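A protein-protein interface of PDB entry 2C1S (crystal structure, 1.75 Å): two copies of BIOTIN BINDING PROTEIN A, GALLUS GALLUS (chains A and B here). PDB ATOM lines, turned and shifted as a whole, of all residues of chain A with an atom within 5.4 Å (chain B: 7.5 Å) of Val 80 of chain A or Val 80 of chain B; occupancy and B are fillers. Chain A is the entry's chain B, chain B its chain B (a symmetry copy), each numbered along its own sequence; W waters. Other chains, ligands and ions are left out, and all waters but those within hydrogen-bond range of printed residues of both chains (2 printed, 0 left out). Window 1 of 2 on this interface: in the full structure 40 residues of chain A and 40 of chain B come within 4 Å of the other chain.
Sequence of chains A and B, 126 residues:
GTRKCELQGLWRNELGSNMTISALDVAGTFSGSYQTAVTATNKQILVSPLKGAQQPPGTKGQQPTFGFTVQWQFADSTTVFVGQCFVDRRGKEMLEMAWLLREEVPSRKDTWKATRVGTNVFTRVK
Of chain B, only Gly 67, Val 80, Phe 81 and Val 82 come within 4 Å of Val 80 of chain A.
Val 80 of chain B touches four residues of chain A.
Printed residues of chain B within 4 Å of Phe 81 of chain A: Val 80 (3.5 Å).
Of the printed residues of chain A, Gly 67 of chain B touches Thr 69, Thr 78 and Val 80.
Printed residues of chain A within 4 Å of Ala 98 of chain B: Leu 100.
Leu 101 of chain B touches none of the printed residues of chain A.
The nearest residue of chain B that does not touch Val 80 of chain A is Phe 68 of chain B (4.2 Å).
The nearest residue of chain A that does not touch Val 80 of chain B is Phe 68 of chain A (4.2 Å).
The nearest printed residue of chain B that does not touch Trp 99 of chain A is Val 80 of chain B (6.3 Å).
Among the printed residues, merely in contact across the chains: Val 80 of chain A with Val 80 of chain B, Val 82 of chain A with Arg 102 of chain B, Phe 81 of chain A with Val 80 of chain B, Val 80 of chain A with Phe 81 of chain B, Thr 78 of chain A with Val 82 of chain B, Val 82 of chain A with Thr 78 of chain B, Trp 99 of chain A with Leu 100 of chain B, Leu 100 of chain A with Trp 99 of chain B, Leu 100 of chain A with Leu 100 of chain B, Val 82 of chain A with Leu 100 of chain B, Leu 100 of chain A with Val 82 of chain B, Ala 98 of chain A with Leu 100 of chain B, Leu 100 of chain A with Ala 98 of chain B, Thr 78 of chain A with Gly 67 of chain B, Gly 67 of chain A with Thr 78 of chain B, Thr 78 of chain A with Phe 66 of chain B, Val 82 of chain A with Val 80 of chain B, Val 80 of chain A with Val 82 of chain B, Gly 67 of chain A with Val 80 of chain B, Val 80 of chain A with Gly 67 of chain B and Ala 98 of chain A with Thr 115 of chain B.
Gly 67 of chain A touches Thr 69 of chain B, and with the chains exchanged Thr 69 of chain A touches Gly 67 of chain B.
Ala 98 of chain A touches Leu 100 of chain B, and with the chains exchanged Leu 100 of chain A touches Ala 98 of chain B.
The backbone NH of Val 82 of chain B lies within hydrogen-bond range of the backbone carbonyl oxygen of Ala 98 of chain B (2.8 Å).
O of Val 80 of chain A lies within hydrogen-bond range of N of Leu 100 of chain A (3.0 Å).
N of Gly 83 of chain B is in hydrogen-bond range of O of Phe 66 of chain B (2.9 Å).
Of the 13 printed residues of chain A, 10 touch a printed residue of chain B.
Printed residues of chain A that touch a printed residue of chain B: Gly 67, Phe 68, Thr 69, Thr 78, Val 80, Phe 81, Val 82, Ala 98, Trp 99 and Leu 100.
Hydrophobic or aromatic side chains of chain A within 4 Å of the printed part of chain B: Val 80, Val 82, Ala 98 and Leu 100.
Hydrophobic or aromatic side chains of chain B within 4 Å of the printed part of chain A: Val 80, Val 82, Ala 98 and Leu 100.
Among the printed residues, 25 pairs touch across the chains.
Among the printed residues, no Asp or Glu carboxylate lies within 4 Å of a Lys or Arg side-chain nitrogen of the other chain.
The side-chain hydroxyl (OG1) of Thr 69 of chain A lies within hydrogen-bond range of the backbone NH (N) of Phe 68 of chain B.
The side-chain hydroxyl of Thr 69 of chain A lies close to the backbone carbonyl oxygen of Gly 67 of chain B.
The backbone NH of Phe 68 of chain A is in hydrogen-bond range of the side-chain hydroxyl of Thr 69 of chain B (3.4 Å).
O of Gly 67 of chain A sits close to OG1 of Thr 69 of chain B, at 3.4 Å.
Water W2 bridges the side-chain hydroxyl of Thr 78 of chain A (2.9 Å) and the backbone carbonyl oxygen of Ala 53 of chain B (3.1 Å).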
ATOM      1  N   GLY A  67     -29.994 -21.132 -10.982  1.00  0.00           N
ATOM      2  CA  GLY A  67     -29.043 -20.227 -11.620  1.00  0.00           C
ATOM      3  C   GLY A  67     -28.457 -20.862 -12.832  1.00  0.00           C
ATOM      4  O   GLY A  67     -28.532 -22.072 -13.004  1.00  0.00           O
ATOM      5  N   PHE A  68     -27.853 -20.043 -13.691  1.00  0.00           N
ATOM      6  CA  PHE A  68     -27.123 -20.579 -14.815  1.00  0.00           C
ATOM      7  C   PHE A  68     -26.063 -19.598 -15.268  1.00  0.00           C
ATOM      8  O   PHE A  68     -26.097 -18.403 -14.894  1.00  0.00           O
ATOM      9  CB  PHE A  68     -28.068 -20.925 -15.997  1.00  0.00           C
ATOM     10  CG  PHE A  68     -28.946 -19.764 -16.477  1.00  0.00           C
ATOM     11  CD1 PHE A  68     -28.502 -18.901 -17.480  1.00  0.00           C
ATOM     12  CD2 PHE A  68     -30.253 -19.599 -15.984  1.00  0.00           C
ATOM     13  CE1 PHE A  68     -29.313 -17.868 -17.951  1.00  0.00           C
ATOM     14  CE2 PHE A  68     -31.063 -18.577 -16.466  1.00  0.00           C
ATOM     15  CZ  PHE A  68     -30.585 -17.695 -17.433  1.00  0.00           C
ATOM     16  N   THR A  69     -25.154 -20.136 -16.077  1.00  0.00           N
ATOM     17  CA  THR A  69     -24.061 -19.416 -16.672  1.00  0.00           C
ATOM     18  C   THR A  69     -24.293 -19.356 -18.185  1.00  0.00           C
ATOM     19  O   THR A  69     -24.487 -20.401 -18.833  1.00  0.00           O
ATOM     20  CB  THR A  69     -22.689 -20.098 -16.361  1.00  0.00           C
ATOM     21  OG1 THR A  69     -22.508 -20.154 -14.940  1.00  0.00           O
ATOM     22  CG2 THR A  69     -21.519 -19.258 -16.973  1.00  0.00           C
ATOM     23  N   VAL A  70     -24.189 -18.153 -18.741  1.00  0.00           N
ATOM     24  CA  VAL A  70     -24.179 -17.974 -20.200  1.00  0.00           C
ATOM     25  C   VAL A  70     -22.759 -17.763 -20.715  1.00  0.00           C
ATOM     26  O   VAL A  70     -22.086 -16.811 -20.332  1.00  0.00           O
ATOM     27  CB  VAL A  70     -25.126 -16.826 -20.644  1.00  0.00           C
ATOM     28  CG1 VAL A  70     -25.239 -16.764 -22.185  1.00  0.00           C
ATOM     29  CG2 VAL A  70     -26.502 -17.057 -20.068  1.00  0.00           C
ATOM     30  N   THR A  78     -18.723 -13.364 -19.555  1.00  0.00           N
ATOM     31  CA  THR A  78     -19.554 -14.434 -19.070  1.00  0.00           C
ATOM     32  C   THR A  78     -20.576 -13.787 -18.172  1.00  0.00           C
ATOM     33  O   THR A  78     -20.259 -12.873 -17.410  1.00  0.00           O
ATOM     34  CB  THR A  78     -18.730 -15.475 -18.241  1.00  0.00           C
ATOM     35  OG1 THR A  78     -17.834 -16.155 -19.116  1.00  0.00           O
ATOM     36  CG2 THR A  78     -19.627 -16.527 -17.562  1.00  0.00           C
ATOM     37  N   THR A  79     -21.814 -14.269 -18.251  1.00  0.00           N
ATOM     38  CA  THR A  79     -22.870 -13.794 -17.363  1.00  0.00           C
ATOM     39  C   THR A  79     -23.403 -14.942 -16.547  1.00  0.00           C
ATOM     40  O   THR A  79     -23.512 -16.083 -17.040  1.00  0.00           O
ATOM     41  CB  THR A  79     -24.093 -13.161 -18.168  1.00  0.00           C
ATOM     42  OG1 THR A  79     -23.630 -12.082 -18.989  1.00  0.00           O
ATOM     43  CG2 THR A  79     -25.206 -12.626 -17.208  1.00  0.00           C
ATOM     44  N   VAL A  80     -23.737 -14.647 -15.294  1.00  0.00           N
ATOM     45  CA  VAL A  80     -24.489 -15.632 -14.526  1.00  0.00           C
ATOM     46  C   VAL A  80     -25.810 -14.978 -14.143  1.00  0.00           C
ATOM     47  O   VAL A  80     -25.874 -13.758 -13.902  1.00  0.00           O
ATOM     48  CB  VAL A  80     -23.711 -16.071 -13.253  1.00  0.00           C
ATOM     49  CG1 VAL A  80     -22.460 -16.927 -13.646  1.00  0.00           C
ATOM     50  CG2 VAL A  80     -23.321 -14.829 -12.411  1.00  0.00           C
ATOM     51  N   PHE A  81     -26.859 -15.791 -14.078  1.00  0.00           N
ATOM     52  CA  PHE A  81     -28.157 -15.309 -13.711  1.00  0.00           C
ATOM     53  C   PHE A  81     -28.599 -16.179 -12.557  1.00  0.00           C
ATOM     54  O   PHE A  81     -28.288 -17.372 -12.550  1.00  0.00           O
ATOM     55  CB  PHE A  81     -29.150 -15.550 -14.853  1.00  0.00           C
ATOM     56  CG  PHE A  81     -28.985 -14.643 -16.054  1.00  0.00           C
ATOM     57  CD1 PHE A  81     -29.872 -13.588 -16.257  1.00  0.00           C
ATOM     58  CD2 PHE A  81     -28.005 -14.901 -17.012  1.00  0.00           C
ATOM     59  CE1 PHE A  81     -29.764 -12.769 -17.430  1.00  0.00           C
ATOM     60  CE2 PHE A  81     -27.877 -14.111 -18.186  1.00  0.00           C
ATOM     61  CZ  PHE A  81     -28.762 -13.012 -18.379  1.00  0.00           C
ATOM     62  N   VAL A  82     -29.312 -15.586 -11.596  1.00  0.00           N
ATOM     63  CA  VAL A  82     -29.891 -16.357 -10.500  1.00  0.00           C
ATOM     64  C   VAL A  82     -31.287 -15.835 -10.194  1.00  0.00           C
ATOM     65  O   VAL A  82     -31.543 -14.632 -10.270  1.00  0.00           O
ATOM     66  CB  VAL A  82     -28.918 -16.352  -9.261  1.00  0.00           C
ATOM     67  CG1 VAL A  82     -28.864 -14.960  -8.590  1.00  0.00           C
ATOM     68  CG2 VAL A  82     -29.234 -17.502  -8.260  1.00  0.00           C
ATOM     69  N   ALA A  98     -31.626 -11.933 -11.110  1.00  0.00           N
ATOM     70  CA  ALA A  98     -30.561 -10.948 -11.008  1.00  0.00           C
ATOM     71  C   ALA A  98     -29.399 -11.562 -11.778  1.00  0.00           C
ATOM     72  O   ALA A  98     -29.313 -12.788 -11.883  1.00  0.00           O
ATOM     73  CB  ALA A  98     -30.180 -10.726  -9.536  1.00  0.00           C
ATOM     74  N   TRP A  99     -28.515 -10.720 -12.287  1.00  0.00           N
ATOM     75  CA  TRP A  99     -27.379 -11.188 -13.072  1.00  0.00           C
ATOM     76  C   TRP A  99     -26.113 -10.412 -12.794  1.00  0.00           C
ATOM     77  O   TRP A  99     -26.164  -9.257 -12.353  1.00  0.00           O
ATOM     78  CB  TRP A  99     -27.698 -11.163 -14.582  1.00  0.00           C
ATOM     79  CG  TRP A  99     -28.189  -9.823 -15.148  1.00  0.00           C
ATOM     80  CD1 TRP A  99     -29.475  -9.464 -15.423  1.00  0.00           C
ATOM     81  CD2 TRP A  99     -27.371  -8.721 -15.533  1.00  0.00           C
ATOM     82  NE1 TRP A  99     -29.503  -8.186 -15.963  1.00  0.00           N
ATOM     83  CE2 TRP A  99     -28.229  -7.701 -16.021  1.00  0.00           C
ATOM     84  CE3 TRP A  99     -25.989  -8.475 -15.471  1.00  0.00           C
ATOM     85  CZ2 TRP A  99     -27.734  -6.460 -16.497  1.00  0.00           C
ATOM     86  CZ3 TRP A  99     -25.498  -7.237 -15.939  1.00  0.00           C
ATOM     87  CH2 TRP A  99     -26.376  -6.253 -16.439  1.00  0.00           C
ATOM     88  N   LEU A 100     -24.987 -11.069 -13.000  1.00  0.00           N
ATOM     89  CA  LEU A 100     -23.702 -10.400 -13.087  1.00  0.00           C
ATOM     90  C   LEU A 100     -23.029 -10.677 -14.436  1.00  0.00           C
ATOM     91  O   LEU A 100     -22.912 -11.825 -14.846  1.00  0.00           O
ATOM     92  CB  LEU A 100     -22.767 -10.909 -12.023  1.00  0.00           C
ATOM     93  CG  LEU A 100     -23.139 -10.719 -10.543  1.00  0.00           C
ATOM     94  CD1 LEU A 100     -22.195 -11.570  -9.638  1.00  0.00           C
ATOM     95  CD2 LEU A 100     -23.145  -9.236 -10.153  1.00  0.00           C
ATOM     96  N   LEU A 101     -22.527  -9.627 -15.077  1.00  0.00           N
ATOM     97  CA  LEU A 101     -21.817  -9.740 -16.359  1.00  0.00           C
ATOM     98  C   LEU A 101     -20.353  -9.419 -16.101  1.00  0.00           C
ATOM     99  O   LEU A 101     -20.020  -8.316 -15.627  1.00  0.00           O
ATOM    100  CB  LEU A 101     -22.453  -8.796 -17.421  1.00  0.00           C
ATOM    101  CG  LEU A 101     -21.672  -8.544 -18.727  1.00  0.00           C
ATOM    102  CD1 LEU A 101     -21.567  -9.808 -19.537  1.00  0.00           C
ATOM    103  CD2 LEU A 101     -22.398  -7.428 -19.509  1.00  0.00           C
ATOM    104  N   LYS B  51     -21.865 -26.324 -11.125  1.00  0.00           N
ATOM    105  CA  LYS B  51     -21.917 -26.591 -12.572  1.00  0.00           C
ATOM    106  C   LYS B  51     -21.621 -25.252 -13.206  1.00  0.00           C
ATOM    107  O   LYS B  51     -22.210 -24.243 -12.833  1.00  0.00           O
ATOM    108  CB  LYS B  51     -23.330 -27.032 -13.033  1.00  0.00           C
ATOM    109  CG  LYS B  51     -23.788 -28.411 -12.548  1.00  0.00           C
ATOM    110  CD  LYS B  51     -22.865 -29.569 -13.029  1.00  0.00           C
ATOM    111  CE  LYS B  51     -23.172 -30.947 -12.379  1.00  0.00           C
ATOM    112  NZ  LYS B  51     -23.476 -30.823 -10.904  1.00  0.00           N
ATOM    113  N   GLY B  52     -20.710 -25.234 -14.164  1.00  0.00           N
ATOM    114  CA  GLY B  52     -20.416 -23.977 -14.833  1.00  0.00           C
ATOM    115  C   GLY B  52     -19.759 -24.160 -16.195  1.00  0.00           C
ATOM    116  O   GLY B  52     -19.734 -25.239 -16.762  1.00  0.00           O
ATOM    117  N   ALA B  53     -19.222 -23.065 -16.689  1.00  0.00           N
ATOM    118  CA  ALA B  53     -18.622 -23.000 -17.998  1.00  0.00           C
ATOM    119  C   ALA B  53     -17.582 -21.896 -18.027  1.00  0.00           C
ATOM    120  O   ALA B  53     -17.739 -20.832 -17.405  1.00  0.00           O
ATOM    121  CB  ALA B  53     -19.716 -22.755 -19.067  1.00  0.00           C
ATOM    122  N   PHE B  66     -15.256 -16.982 -16.489  1.00  0.00           N
ATOM    123  CA  PHE B  66     -15.974 -18.201 -16.188  1.00  0.00           C
ATOM    124  C   PHE B  66     -17.050 -17.930 -15.151  1.00  0.00           C
ATOM    125  O   PHE B  66     -17.017 -16.929 -14.449  1.00  0.00           O
ATOM    126  CB  PHE B  66     -15.076 -19.335 -15.691  1.00  0.00           C
ATOM    127  CG  PHE B  66     -14.388 -19.054 -14.395  1.00  0.00           C
ATOM    128  CD1 PHE B  66     -14.871 -19.596 -13.208  1.00  0.00           C
ATOM    129  CD2 PHE B  66     -13.242 -18.255 -14.354  1.00  0.00           C
ATOM    130  CE1 PHE B  66     -14.222 -19.349 -11.973  1.00  0.00           C
ATOM    131  CE2 PHE B  66     -12.593 -17.984 -13.138  1.00  0.00           C
ATOM    132  CZ  PHE B  66     -13.075 -18.537 -11.948  1.00  0.00           C
ATOM    133  N   GLY B  67     -18.002 -18.835 -15.078  1.00  0.00           N
ATOM    134  CA  GLY B  67     -19.000 -18.743 -14.015  1.00  0.00           C
ATOM    135  C   GLY B  67     -19.493 -20.098 -13.651  1.00  0.00           C
ATOM    136  O   GLY B  67     -19.318 -21.053 -14.398  1.00  0.00           O
ATOM    137  N   PHE B  68     -20.131 -20.197 -12.485  1.00  0.00           N
ATOM    138  CA  PHE B  68     -20.779 -21.433 -12.114  1.00  0.00           C
ATOM    139  C   PHE B  68     -21.896 -21.164 -11.130  1.00  0.00           C
ATOM    140  O   PHE B  68     -21.968 -20.068 -10.529  1.00  0.00           O
ATOM    141  CB  PHE B  68     -19.771 -22.447 -11.511  1.00  0.00           C
ATOM    142  CG  PHE B  68     -18.970 -21.921 -10.314  1.00  0.00           C
ATOM    143  CD1 PHE B  68     -19.447 -22.081  -9.012  1.00  0.00           C
ATOM    144  CD2 PHE B  68     -17.698 -21.351 -10.494  1.00  0.00           C
ATOM    145  CE1 PHE B  68     -18.705 -21.642  -7.915  1.00  0.00           C
ATOM    146  CE2 PHE B  68     -16.955 -20.928  -9.397  1.00  0.00           C
ATOM    147  CZ  PHE B  68     -17.468 -21.051  -8.108  1.00  0.00           C
ATOM    148  N   THR B  69     -22.733 -22.188 -10.985  1.00  0.00           N
ATOM    149  CA  THR B  69     -23.859 -22.205 -10.091  1.00  0.00           C
ATOM    150  C   THR B  69     -23.582 -23.232  -8.989  1.00  0.00           C
ATOM    151  O   THR B  69     -23.285 -24.405  -9.284  1.00  0.00           O
ATOM    152  CB  THR B  69     -25.183 -22.560 -10.843  1.00  0.00           C
ATOM    153  OG1 THR B  69     -25.406 -21.590 -11.876  1.00  0.00           O
ATOM    154  CG2 THR B  69     -26.394 -22.510  -9.853  1.00  0.00           C
ATOM    155  N   VAL B  70     -23.761 -22.809  -7.742  1.00  0.00           N
ATOM    156  CA  VAL B  70     -23.736 -23.735  -6.600  1.00  0.00           C
ATOM    157  C   VAL B  70     -25.150 -24.071  -6.139  1.00  0.00           C
ATOM    158  O   VAL B  70     -25.909 -23.190  -5.743  1.00  0.00           O
ATOM    159  CB  VAL B  70     -22.868 -23.187  -5.435  1.00  0.00           C
ATOM    160  CG1 VAL B  70     -22.710 -24.243  -4.317  1.00  0.00           C
ATOM    161  CG2 VAL B  70     -21.499 -22.824  -5.956  1.00  0.00           C
ATOM    162  N   TRP B  72     -26.839 -25.526  -3.331  1.00  0.00           N
ATOM    163  CA  TRP B  72     -26.562 -25.809  -1.922  1.00  0.00           C
ATOM    164  C   TRP B  72     -27.392 -27.001  -1.425  1.00  0.00           C
ATOM    165  O   TRP B  72     -28.576 -27.125  -1.709  1.00  0.00           O
ATOM    166  CB  TRP B  72     -26.799 -24.567  -1.045  1.00  0.00           C
ATOM    167  CG  TRP B  72     -25.986 -23.376  -1.461  1.00  0.00           C
ATOM    168  CD1 TRP B  72     -26.450 -22.246  -2.029  1.00  0.00           C
ATOM    169  CD2 TRP B  72     -24.566 -23.214  -1.326  1.00  0.00           C
ATOM    170  NE1 TRP B  72     -25.415 -21.379  -2.289  1.00  0.00           N
ATOM    171  CE2 TRP B  72     -24.241 -21.939  -1.860  1.00  0.00           C
ATOM    172  CE3 TRP B  72     -23.540 -24.026  -0.822  1.00  0.00           C
ATOM    173  CZ2 TRP B  72     -22.937 -21.447  -1.902  1.00  0.00           C
ATOM    174  CZ3 TRP B  72     -22.227 -23.530  -0.840  1.00  0.00           C
ATOM    175  CH2 TRP B  72     -21.940 -22.241  -1.380  1.00  0.00           C
ATOM    176  N   THR B  78     -29.556 -20.515  -3.916  1.00  0.00           N
ATOM    177  CA  THR B  78     -28.660 -20.839  -4.995  1.00  0.00           C
ATOM    178  C   THR B  78     -27.722 -19.667  -5.119  1.00  0.00           C
ATOM    179  O   THR B  78     -28.135 -18.513  -5.001  1.00  0.00           O
ATOM    180  CB  THR B  78     -29.427 -21.028  -6.346  1.00  0.00           C
ATOM    181  OG1 THR B  78     -30.237 -22.196  -6.257  1.00  0.00           O
ATOM    182  CG2 THR B  78     -28.474 -21.196  -7.543  1.00  0.00           C
ATOM    183  N   THR B  79     -26.448 -19.960  -5.369  1.00  0.00           N
ATOM    184  CA  THR B  79     -25.463 -18.910  -5.610  1.00  0.00           C
ATOM    185  C   THR B  79     -24.870 -19.075  -6.983  1.00  0.00           C
ATOM    186  O   THR B  79     -24.655 -20.209  -7.458  1.00  0.00           O
ATOM    187  CB  THR B  79     -24.267 -18.956  -4.555  1.00  0.00           C
ATOM    188  OG1 THR B  79     -24.786 -18.837  -3.224  1.00  0.00           O
ATOM    189  CG2 THR B  79     -23.232 -17.809  -4.800  1.00  0.00           C
ATOM    190  N   VAL B  80     -24.601 -17.945  -7.630  1.00  0.00           N
ATOM    191  CA  VAL B  80     -23.800 -18.014  -8.847  1.00  0.00           C
ATOM    192  C   VAL B  80     -22.548 -17.184  -8.598  1.00  0.00           C
ATOM    193  O   VAL B  80     -22.588 -16.162  -7.887  1.00  0.00           O
ATOM    194  CB  VAL B  80     -24.583 -17.464 -10.072  1.00  0.00           C
ATOM    195  CG1 VAL B  80     -25.750 -18.436 -10.457  1.00  0.00           C
ATOM    196  CG2 VAL B  80     -25.098 -16.031  -9.777  1.00  0.00           C
ATOM    197  N   PHE B  81     -21.441 -17.616  -9.193  1.00  0.00           N
ATOM    198  CA  PHE B  81     -20.198 -16.918  -9.059  1.00  0.00           C
ATOM    199  C   PHE B  81     -19.728 -16.654 -10.470  1.00  0.00           C
ATOM    200  O   PHE B  81     -19.945 -17.498 -11.343  1.00  0.00           O
ATOM    201  CB  PHE B  81     -19.152 -17.827  -8.406  1.00  0.00           C
ATOM    202  CG  PHE B  81     -19.347 -18.077  -6.925  1.00  0.00           C
ATOM    203  CD1 PHE B  81     -18.540 -17.424  -5.996  1.00  0.00           C
ATOM    204  CD2 PHE B  81     -20.271 -19.021  -6.478  1.00  0.00           C
ATOM    205  CE1 PHE B  81     -18.672 -17.710  -4.596  1.00  0.00           C
ATOM    206  CE2 PHE B  81     -20.422 -19.329  -5.098  1.00  0.00           C
ATOM    207  CZ  PHE B  81     -19.620 -18.638  -4.146  1.00  0.00           C
ATOM    208  N   VAL B  82     -19.097 -15.498 -10.687  1.00  0.00           N
ATOM    209  CA  VAL B  82     -18.496 -15.198 -11.984  1.00  0.00           C
ATOM    210  C   VAL B  82     -17.156 -14.508 -11.774  1.00  0.00           C
ATOM    211  O   VAL B  82     -16.993 -13.712 -10.849  1.00  0.00           O
ATOM    212  CB  VAL B  82     -19.506 -14.380 -12.873  1.00  0.00           C
ATOM    213  CG1 VAL B  82     -19.692 -12.940 -12.341  1.00  0.00           C
ATOM    214  CG2 VAL B  82     -19.135 -14.430 -14.384  1.00  0.00           C
ATOM    215  N   GLY B  83     -16.182 -14.811 -12.641  1.00  0.00           N
ATOM    216  CA  GLY B  83     -14.832 -14.387 -12.371  1.00  0.00           C
ATOM    217  C   GLY B  83     -13.802 -14.625 -13.470  1.00  0.00           C
ATOM    218  O   GLY B  83     -14.113 -14.942 -14.630  1.00  0.00           O
ATOM    219  N   MET B  97     -13.539 -13.243  -7.982  1.00  0.00           N
ATOM    220  CA  MET B  97     -14.956 -13.602  -8.244  1.00  0.00           C
ATOM    221  C   MET B  97     -15.964 -12.625  -7.639  1.00  0.00           C
ATOM    222  O   MET B  97     -15.698 -12.000  -6.623  1.00  0.00           O
ATOM    223  CB  MET B  97     -15.275 -15.030  -7.804  1.00  0.00           C
ATOM    224  CG  MET B  97     -14.331 -16.063  -8.464  1.00  0.00           C
ATOM    225  SD  MET B  97     -15.107 -17.664  -8.700  1.00  0.00           S
ATOM    226  CE  MET B  97     -15.962 -17.341 -10.250  1.00  0.00           C
ATOM    227  N   ALA B  98     -17.093 -12.444  -8.323  1.00  0.00           N
ATOM    228  CA  ALA B  98     -18.235 -11.774  -7.721  1.00  0.00           C
ATOM    229  C   ALA B  98     -19.319 -12.843  -7.667  1.00  0.00           C
ATOM    230  O   ALA B  98     -19.305 -13.772  -8.478  1.00  0.00           O
ATOM    231  CB  ALA B  98     -18.681 -10.592  -8.596  1.00  0.00           C
ATOM    232  N   TRP B  99     -20.249 -12.696  -6.737  1.00  0.00           N
ATOM    233  CA  TRP B  99     -21.318 -13.673  -6.566  1.00  0.00           C
ATOM    234  C   TRP B  99     -22.649 -13.037  -6.243  1.00  0.00           C
ATOM    235  O   TRP B  99     -22.704 -11.917  -5.718  1.00  0.00           O
ATOM    236  CB  TRP B  99     -20.951 -14.715  -5.489  1.00  0.00           C
ATOM    237  CG  TRP B  99     -20.548 -14.159  -4.117  1.00  0.00           C
ATOM    238  CD1 TRP B  99     -19.286 -14.007  -3.624  1.00  0.00           C
ATOM    239  CD2 TRP B  99     -21.438 -13.738  -3.084  1.00  0.00           C
ATOM    240  NE1 TRP B  99     -19.341 -13.511  -2.329  1.00  0.00           N
ATOM    241  CE2 TRP B  99     -20.646 -13.317  -1.984  1.00  0.00           C
ATOM    242  CE3 TRP B  99     -22.835 -13.632  -2.996  1.00  0.00           C
ATOM    243  CZ2 TRP B  99     -21.221 -12.840  -0.777  1.00  0.00           C
ATOM    244  CZ3 TRP B  99     -23.407 -13.152  -1.798  1.00  0.00           C
ATOM    245  CH2 TRP B  99     -22.592 -12.762  -0.714  1.00  0.00           C
ATOM    246  N   LEU B 100     -23.713 -13.726  -6.610  1.00  0.00           N
ATOM    247  CA  LEU B 100     -25.043 -13.428  -6.111  1.00  0.00           C
ATOM    248  C   LEU B 100     -25.647 -14.641  -5.396  1.00  0.00           C
ATOM    249  O   LEU B 100     -25.660 -15.738  -5.941  1.00  0.00           O
ATOM    250  CB  LEU B 100     -25.970 -13.088  -7.248  1.00  0.00           C
ATOM    251  CG  LEU B 100     -25.663 -11.863  -8.127  1.00  0.00           C
ATOM    252  CD1 LEU B 100     -26.568 -11.875  -9.399  1.00  0.00           C
ATOM    253  CD2 LEU B 100     -25.787 -10.559  -7.331  1.00  0.00           C
ATOM    254  N   LEU B 101     -26.208 -14.416  -4.213  1.00  0.00           N
ATOM    255  CA  LEU B 101     -26.864 -15.471  -3.427  1.00  0.00           C
ATOM    256  C   LEU B 101     -28.356 -15.179  -3.425  1.00  0.00           C
ATOM    257  O   LEU B 101     -28.790 -14.103  -2.973  1.00  0.00           O
ATOM    258  CB  LEU B 101     -26.268 -15.532  -1.991  1.00  0.00           C
ATOM    259  CG  LEU B 101     -27.022 -16.359  -0.929  1.00  0.00           C
ATOM    260  CD1 LEU B 101     -27.002 -17.822  -1.278  1.00  0.00           C
ATOM    261  CD2 LEU B 101     -26.361 -16.093   0.441  1.00  0.00           C
ATOM    262  N   ARG B 102     -29.128 -16.097  -3.988  1.00  0.00           N
ATOM    263  CA  ARG B 102     -30.574 -15.910  -4.143  1.00  0.00           C
ATOM    264  C   ARG B 102     -31.294 -16.789  -3.155  1.00  0.00           C
ATOM    265  O   ARG B 102     -31.111 -18.024  -3.164  1.00  0.00           O
ATOM    266  CB  ARG B 102     -31.011 -16.313  -5.549  1.00  0.00           C
ATOM    267  CG  ARG B 102     -32.523 -16.171  -5.888  1.00  0.00           C
ATOM    268  CD  ARG B 102     -33.102 -14.826  -5.510  1.00  0.00           C
ATOM    269  NE  ARG B 102     -34.421 -14.439  -6.075  1.00  0.00           N
ATOM    270  CZ  ARG B 102     -35.614 -14.898  -5.689  1.00  0.00           C
ATOM    271  NH1 ARG B 102     -35.715 -15.824  -4.762  1.00  0.00           N
ATOM    272  NH2 ARG B 102     -36.725 -14.407  -6.236  1.00  0.00           N
ATOM    273  N   THR B 115     -31.858 -11.152  -2.985  1.00  0.00           N
ATOM    274  CA  THR B 115     -30.534 -11.361  -3.602  1.00  0.00           C
ATOM    275  C   THR B 115     -29.461 -10.564  -2.907  1.00  0.00           C
ATOM    276  O   THR B 115     -29.537  -9.345  -2.871  1.00  0.00           O
ATOM    277  CB  THR B 115     -30.532 -10.882  -5.062  1.00  0.00           C
ATOM    278  OG1 THR B 115     -31.649 -11.451  -5.758  1.00  0.00           O
ATOM    279  CG2 THR B 115     -29.241 -11.323  -5.763  1.00  0.00           C
ATOM    280  N   ARG B 116     -28.472 -11.260  -2.366  1.00  0.00           N
ATOM    281  CA  ARG B 116     -27.308 -10.656  -1.805  1.00  0.00           C
ATOM    282  C   ARG B 116     -26.172 -10.741  -2.842  1.00  0.00           C
ATOM    283  O   ARG B 116     -26.176 -11.588  -3.748  1.00  0.00           O
ATOM    284  CB  ARG B 116     -26.875 -11.393  -0.546  1.00  0.00           C
ATOM    285  CG  ARG B 116     -27.848 -11.375   0.653  1.00  0.00           C
ATOM    286  CD  ARG B 116     -27.057 -12.183   1.716  1.00  0.00           C
ATOM    287  NE  ARG B 116     -27.596 -12.182   3.068  1.00  0.00           N
ATOM    288  CZ  ARG B 116     -28.485 -13.063   3.509  1.00  0.00           C
ATOM    289  NH1 ARG B 116     -28.964 -13.979   2.686  1.00  0.00           N
ATOM    290  NH2 ARG B 116     -28.898 -13.021   4.773  1.00  0.00           N
ATOM    291  N   GLY B 118     -21.676 -10.058  -3.331  1.00  0.00           N
ATOM    292  CA  GLY B 118     -20.362  -9.952  -2.708  1.00  0.00           C
ATOM    293  C   GLY B 118     -19.252 -10.323  -3.674  1.00  0.00           C
ATOM    294  O   GLY B 118     -19.478 -10.535  -4.894  1.00  0.00           O
HETATM  295  O   HOH W   1     -23.882 -22.499 -14.104  1.00  0.00           O
HETATM  296  O   HOH W   2     -18.325 -18.919 -19.726  1.00  0.00           O
